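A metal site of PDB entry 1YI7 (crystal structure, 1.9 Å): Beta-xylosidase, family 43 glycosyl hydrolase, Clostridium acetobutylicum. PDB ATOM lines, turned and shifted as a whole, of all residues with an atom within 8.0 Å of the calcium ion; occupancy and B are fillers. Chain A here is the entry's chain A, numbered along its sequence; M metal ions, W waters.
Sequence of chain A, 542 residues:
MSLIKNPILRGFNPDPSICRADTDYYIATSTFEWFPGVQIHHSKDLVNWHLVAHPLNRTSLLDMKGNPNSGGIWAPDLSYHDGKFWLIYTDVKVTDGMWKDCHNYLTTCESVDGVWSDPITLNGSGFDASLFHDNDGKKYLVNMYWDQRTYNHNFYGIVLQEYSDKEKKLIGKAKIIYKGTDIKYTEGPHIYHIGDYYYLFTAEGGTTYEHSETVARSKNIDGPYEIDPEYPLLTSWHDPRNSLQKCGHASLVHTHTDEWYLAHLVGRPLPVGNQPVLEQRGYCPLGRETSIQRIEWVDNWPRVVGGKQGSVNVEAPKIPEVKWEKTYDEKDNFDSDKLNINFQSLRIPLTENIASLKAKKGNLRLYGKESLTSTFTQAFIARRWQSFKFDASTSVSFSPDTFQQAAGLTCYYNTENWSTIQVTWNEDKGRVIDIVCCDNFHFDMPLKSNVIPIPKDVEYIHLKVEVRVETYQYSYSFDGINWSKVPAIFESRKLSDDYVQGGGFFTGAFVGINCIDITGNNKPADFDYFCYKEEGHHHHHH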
ATOM      1  N   LYS A 331      -4.369 -27.218 -19.947  1.00  0.00           N
ATOM      2  CA  LYS A 331      -5.579 -27.076 -19.138  1.00  0.00           C
ATOM      3  C   LYS A 331      -5.846 -28.396 -18.452  1.00  0.00           C
ATOM      4  O   LYS A 331      -6.274 -29.350 -19.065  1.00  0.00           O
ATOM      5  CB  LYS A 331      -6.809 -26.728 -19.978  1.00  0.00           C
ATOM      6  CG  LYS A 331      -8.068 -26.426 -19.169  1.00  0.00           C
ATOM      7  CD  LYS A 331      -8.982 -25.509 -19.987  1.00  0.00           C
ATOM      8  CE  LYS A 331     -10.259 -25.099 -19.254  1.00  0.00           C
ATOM      9  NZ  LYS A 331     -11.409 -26.004 -19.530  1.00  0.00           N
ATOM     10  N   ASP A 332      -5.616 -28.396 -17.148  1.00  0.00           N
ATOM     11  CA  ASP A 332      -5.848 -29.557 -16.317  1.00  0.00           C
ATOM     12  C   ASP A 332      -7.274 -29.433 -15.804  1.00  0.00           C
ATOM     13  O   ASP A 332      -7.591 -28.526 -15.044  1.00  0.00           O
ATOM     14  CB  ASP A 332      -4.840 -29.541 -15.159  1.00  0.00           C
ATOM     15  CG  ASP A 332      -4.946 -30.761 -14.298  1.00  0.00           C
ATOM     16  OD1 ASP A 332      -5.986 -31.465 -14.413  1.00  0.00           O
ATOM     17  OD2 ASP A 332      -4.067 -31.085 -13.472  1.00  0.00           O
ATOM     18  N   ASN A 333      -8.137 -30.346 -16.225  1.00  0.00           N
ATOM     19  CA  ASN A 333      -9.551 -30.265 -15.889  1.00  0.00           C
ATOM     20  C   ASN A 333      -9.865 -31.039 -14.639  1.00  0.00           C
ATOM     21  O   ASN A 333     -11.044 -31.193 -14.274  1.00  0.00           O
ATOM     22  CB  ASN A 333     -10.447 -30.760 -17.046  1.00  0.00           C
ATOM     23  CG  ASN A 333     -10.374 -29.864 -18.248  1.00  0.00           C
ATOM     24  OD1 ASN A 333     -10.012 -30.291 -19.355  1.00  0.00           O
ATOM     25  ND2 ASN A 333     -10.707 -28.609 -18.041  1.00  0.00           N
ATOM     26  N   PHE A 334      -8.834 -31.600 -14.002  1.00  0.00           N
ATOM     27  CA  PHE A 334      -9.046 -32.292 -12.714  1.00  0.00           C
ATOM     28  C   PHE A 334     -10.056 -33.441 -12.845  1.00  0.00           C
ATOM     29  O   PHE A 334     -10.861 -33.684 -11.933  1.00  0.00           O
ATOM     30  CB  PHE A 334      -9.527 -31.283 -11.658  1.00  0.00           C
ATOM     31  CG  PHE A 334      -8.447 -30.331 -11.193  1.00  0.00           C
ATOM     32  CD1 PHE A 334      -7.173 -30.812 -10.883  1.00  0.00           C
ATOM     33  CD2 PHE A 334      -8.711 -28.975 -11.034  1.00  0.00           C
ATOM     34  CE1 PHE A 334      -6.166 -29.923 -10.424  1.00  0.00           C
ATOM     35  CE2 PHE A 334      -7.719 -28.084 -10.559  1.00  0.00           C
ATOM     36  CZ  PHE A 334      -6.430 -28.544 -10.275  1.00  0.00           C
ATOM     37  N   ASP A 335     -10.010 -34.111 -13.994  1.00  0.00           N
ATOM     38  CA  ASP A 335     -10.855 -35.259 -14.323  1.00  0.00           C
ATOM     39  C   ASP A 335     -10.205 -36.570 -13.947  1.00  0.00           C
ATOM     40  O   ASP A 335     -10.757 -37.619 -14.204  1.00  0.00           O
ATOM     41  CB  ASP A 335     -11.088 -35.305 -15.830  1.00  0.00           C
ATOM     42  CG  ASP A 335     -12.102 -34.301 -16.298  1.00  0.00           C
ATOM     43  OD1 ASP A 335     -13.075 -34.005 -15.562  1.00  0.00           O
ATOM     44  OD2 ASP A 335     -12.011 -33.754 -17.421  1.00  0.00           O
ATOM     45  N   SER A 336      -9.012 -36.518 -13.381  1.00  0.00           N
ATOM     46  CA  SER A 336      -8.321 -37.721 -12.956  1.00  0.00           C
ATOM     47  C   SER A 336      -8.193 -37.634 -11.462  1.00  0.00           C
ATOM     48  O   SER A 336      -8.138 -36.530 -10.907  1.00  0.00           O
ATOM     49  CB  SER A 336      -6.940 -37.774 -13.598  1.00  0.00           C
ATOM     50  OG  SER A 336      -6.109 -38.710 -12.947  1.00  0.00           O
ATOM     51  N   LYS A 360     -15.896 -34.510  -5.632  1.00  0.00           N
ATOM     52  CA  LYS A 360     -16.670 -34.057  -6.789  1.00  0.00           C
ATOM     53  C   LYS A 360     -15.866 -34.196  -8.063  1.00  0.00           C
ATOM     54  O   LYS A 360     -14.940 -33.434  -8.313  1.00  0.00           O
ATOM     55  CB  LYS A 360     -17.139 -32.623  -6.633  1.00  0.00           C
ATOM     56  CG  LYS A 360     -17.951 -32.105  -7.810  1.00  0.00           C
ATOM     57  CD  LYS A 360     -18.672 -30.803  -7.481  1.00  0.00           C
ATOM     58  CE  LYS A 360     -19.602 -30.382  -8.627  1.00  0.00           C
ATOM     59  NZ  LYS A 360     -20.397 -29.161  -8.316  1.00  0.00           N
ATOM     60  N   LYS A 361     -16.270 -35.160  -8.890  1.00  0.00           N
ATOM     61  CA  LYS A 361     -15.620 -35.480 -10.139  1.00  0.00           C
ATOM     62  C   LYS A 361     -15.432 -34.251 -11.003  1.00  0.00           C
ATOM     63  O   LYS A 361     -16.320 -33.420 -11.117  1.00  0.00           O
ATOM     64  CB  LYS A 361     -16.476 -36.522 -10.868  1.00  0.00           C
ATOM     65  CG  LYS A 361     -15.988 -36.905 -12.249  1.00  0.00           C
ATOM     66  CD  LYS A 361     -14.725 -37.739 -12.176  1.00  0.00           C
ATOM     67  CE  LYS A 361     -14.091 -37.860 -13.550  1.00  0.00           C
ATOM     68  NZ  LYS A 361     -12.953 -38.803 -13.503  1.00  0.00           N
ATOM     69  N   GLY A 362     -14.269 -34.138 -11.661  1.00  0.00           N
ATOM     70  CA  GLY A 362     -13.974 -32.975 -12.481  1.00  0.00           C
ATOM     71  C   GLY A 362     -13.617 -31.725 -11.670  1.00  0.00           C
ATOM     72  O   GLY A 362     -13.498 -30.632 -12.225  1.00  0.00           O
ATOM     73  N   ASN A 363     -13.462 -31.883 -10.355  1.00  0.00           N
ATOM     74  CA  ASN A 363     -13.044 -30.770  -9.496  1.00  0.00           C
ATOM     75  C   ASN A 363     -11.957 -31.194  -8.497  1.00  0.00           C
ATOM     76  O   ASN A 363     -11.956 -32.309  -8.029  1.00  0.00           O
ATOM     77  CB  ASN A 363     -14.215 -30.181  -8.680  1.00  0.00           C
ATOM     78  CG  ASN A 363     -15.216 -29.424  -9.522  1.00  0.00           C
ATOM     79  OD1 ASN A 363     -15.385 -28.215  -9.388  1.00  0.00           O
ATOM     80  ND2 ASN A 363     -15.907 -30.136 -10.406  1.00  0.00           N
ATOM     81  N   LEU A 364     -11.063 -30.243  -8.201  1.00  0.00           N
ATOM     82  CA  LEU A 364     -10.225 -30.266  -7.029  1.00  0.00           C
ATOM     83  C   LEU A 364     -10.931 -29.477  -5.899  1.00  0.00           C
ATOM     84  O   LEU A 364     -11.118 -28.249  -5.962  1.00  0.00           O
ATOM     85  CB  LEU A 364      -8.849 -29.644  -7.311  1.00  0.00           C
ATOM     86  CG  LEU A 364      -8.004 -29.694  -6.021  1.00  0.00           C
ATOM     87  CD1 LEU A 364      -7.753 -31.143  -5.596  1.00  0.00           C
ATOM     88  CD2 LEU A 364      -6.690 -28.957  -6.171  1.00  0.00           C
ATOM     89  N   SER A 395     -10.661 -21.717 -12.031  1.00  0.00           N
ATOM     90  CA  SER A 395     -11.945 -21.131 -11.676  1.00  0.00           C
ATOM     91  C   SER A 395     -12.438 -21.814 -10.430  1.00  0.00           C
ATOM     92  O   SER A 395     -12.175 -22.989 -10.214  1.00  0.00           O
ATOM     93  CB  SER A 395     -12.970 -21.208 -12.809  1.00  0.00           C
ATOM     94  OG  SER A 395     -13.404 -22.539 -12.994  1.00  0.00           O
ATOM     95  N   TYR A 460     -18.900 -20.357 -10.770  1.00  0.00           N
ATOM     96  CA  TYR A 460     -17.445 -20.428 -10.784  1.00  0.00           C
ATOM     97  C   TYR A 460     -16.903 -19.068 -11.133  1.00  0.00           C
ATOM     98  O   TYR A 460     -17.307 -18.506 -12.138  1.00  0.00           O
ATOM     99  CB  TYR A 460     -16.942 -21.468 -11.802  1.00  0.00           C
ATOM    100  CG  TYR A 460     -17.102 -22.878 -11.294  1.00  0.00           C
ATOM    101  CD1 TYR A 460     -18.336 -23.534 -11.378  1.00  0.00           C
ATOM    102  CD2 TYR A 460     -16.051 -23.545 -10.685  1.00  0.00           C
ATOM    103  CE1 TYR A 460     -18.492 -24.808 -10.884  1.00  0.00           C
ATOM    104  CE2 TYR A 460     -16.188 -24.834 -10.197  1.00  0.00           C
ATOM    105  CZ  TYR A 460     -17.417 -25.458 -10.298  1.00  0.00           C
ATOM    106  OH  TYR A 460     -17.564 -26.734  -9.802  1.00  0.00           O
ATOM    107  N   PHE A 527     -12.264 -26.210  -7.378  1.00  0.00           N
ATOM    108  CA  PHE A 527     -11.572 -25.644  -8.539  1.00  0.00           C
ATOM    109  C   PHE A 527     -11.853 -26.554  -9.723  1.00  0.00           C
ATOM    110  O   PHE A 527     -11.612 -27.764  -9.674  1.00  0.00           O
ATOM    111  CB  PHE A 527     -10.051 -25.474  -8.290  1.00  0.00           C
ATOM    112  CG  PHE A 527      -9.734 -24.571  -7.125  1.00  0.00           C
ATOM    113  CD1 PHE A 527      -9.841 -25.044  -5.815  1.00  0.00           C
ATOM    114  CD2 PHE A 527      -9.354 -23.250  -7.319  1.00  0.00           C
ATOM    115  CE1 PHE A 527      -9.567 -24.215  -4.720  1.00  0.00           C
ATOM    116  CE2 PHE A 527      -9.073 -22.420  -6.242  1.00  0.00           C
ATOM    117  CZ  PHE A 527      -9.189 -22.913  -4.925  1.00  0.00           C
ATOM    118  N   ASP A 528     -12.385 -25.952 -10.771  1.00  0.00           N
ATOM    119  CA  ASP A 528     -12.808 -26.700 -11.935  1.00  0.00           C
ATOM    120  C   ASP A 528     -11.605 -26.996 -12.836  1.00  0.00           C
ATOM    121  O   ASP A 528     -11.598 -27.958 -13.576  1.00  0.00           O
ATOM    122  CB  ASP A 528     -13.854 -25.919 -12.717  1.00  0.00           C
ATOM    123  CG  ASP A 528     -14.360 -26.692 -13.921  1.00  0.00           C
ATOM    124  OD1 ASP A 528     -14.725 -27.860 -13.727  1.00  0.00           O
ATOM    125  OD2 ASP A 528     -14.409 -26.248 -15.085  1.00  0.00           O
ATOM    126  N   TYR A 529     -10.601 -26.154 -12.813  1.00  0.00           N
ATOM    127  CA  TYR A 529      -9.480 -26.454 -13.669  1.00  0.00           C
ATOM    128  C   TYR A 529      -8.263 -25.678 -13.185  1.00  0.00           C
ATOM    129  O   TYR A 529      -8.410 -24.739 -12.377  1.00  0.00           O
ATOM    130  CB  TYR A 529      -9.813 -26.122 -15.144  1.00  0.00           C
ATOM    131  CG  TYR A 529     -10.041 -24.648 -15.412  1.00  0.00           C
ATOM    132  CD1 TYR A 529      -8.957 -23.789 -15.616  1.00  0.00           C
ATOM    133  CD2 TYR A 529     -11.344 -24.116 -15.488  1.00  0.00           C
ATOM    134  CE1 TYR A 529      -9.149 -22.420 -15.864  1.00  0.00           C
ATOM    135  CE2 TYR A 529     -11.550 -22.746 -15.721  1.00  0.00           C
ATOM    136  CZ  TYR A 529     -10.433 -21.899 -15.903  1.00  0.00           C
ATOM    137  OH  TYR A 529     -10.584 -20.551 -16.160  1.00  0.00           O
ATOM    138  N   PHE A 530      -7.087 -26.072 -13.665  1.00  0.00           N
ATOM    139  CA  PHE A 530      -5.883 -25.238 -13.522  1.00  0.00           C
ATOM    140  C   PHE A 530      -5.115 -25.181 -14.865  1.00  0.00           C
ATOM    141  O   PHE A 530      -4.690 -26.209 -15.402  1.00  0.00           O
ATOM    142  CB  PHE A 530      -4.979 -25.754 -12.387  1.00  0.00           C
ATOM    143  CG  PHE A 530      -3.803 -24.849 -12.092  1.00  0.00           C
ATOM    144  CD1 PHE A 530      -3.938 -23.788 -11.202  1.00  0.00           C
ATOM    145  CD2 PHE A 530      -2.586 -25.035 -12.731  1.00  0.00           C
ATOM    146  CE1 PHE A 530      -2.859 -22.936 -10.932  1.00  0.00           C
ATOM    147  CE2 PHE A 530      -1.503 -24.183 -12.470  1.00  0.00           C
ATOM    148  CZ  PHE A 530      -1.650 -23.142 -11.564  1.00  0.00           C
HETATM  149 CA    CA M   1     -12.980 -29.723 -14.299  1.00  0.00          CA
HETATM  150  O   HOH W   1     -12.935 -28.530 -16.535  1.00  0.00           O
HETATM  151  O   HOH W   2     -14.621 -31.285 -15.579  1.00  0.00           O
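N of Gly 362 sits close to O of Phe 334, 3.4 Å away.
The backbone carbonyl oxygen (O) of Ser 395 is in hydrogen-bond range of the backbone NH (N) of Asp 528.
ND2 of Asn 333 lies close to NZ of Lys 331 (3.1 Å).
Three residues have an atom within 4 Å of the calcium ion: Asn 333, Gly 362 and Asp 528.
The calcium ion is bound by O of Gly 362, at 2.3 Å.
The calcium ion is bound by O of Asp 528, at 2.4 Å.
O of Asn 333 binds the calcium ion (2.4 Å).
Water W1 is bound to the calcium ion (2.5 Å).
The calcium ion is bound by water W2, 2.6 Å away.
OD1 of Asp 528 is bound to the calcium ion, at 2.6 Å.
The calcium ion has six donor atoms within binding distance.
Water W1 lies within hydrogen-bond range of ND2 of Asn 333 (2.7 Å) and OD2 of Asp 528 (3.1 Å).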
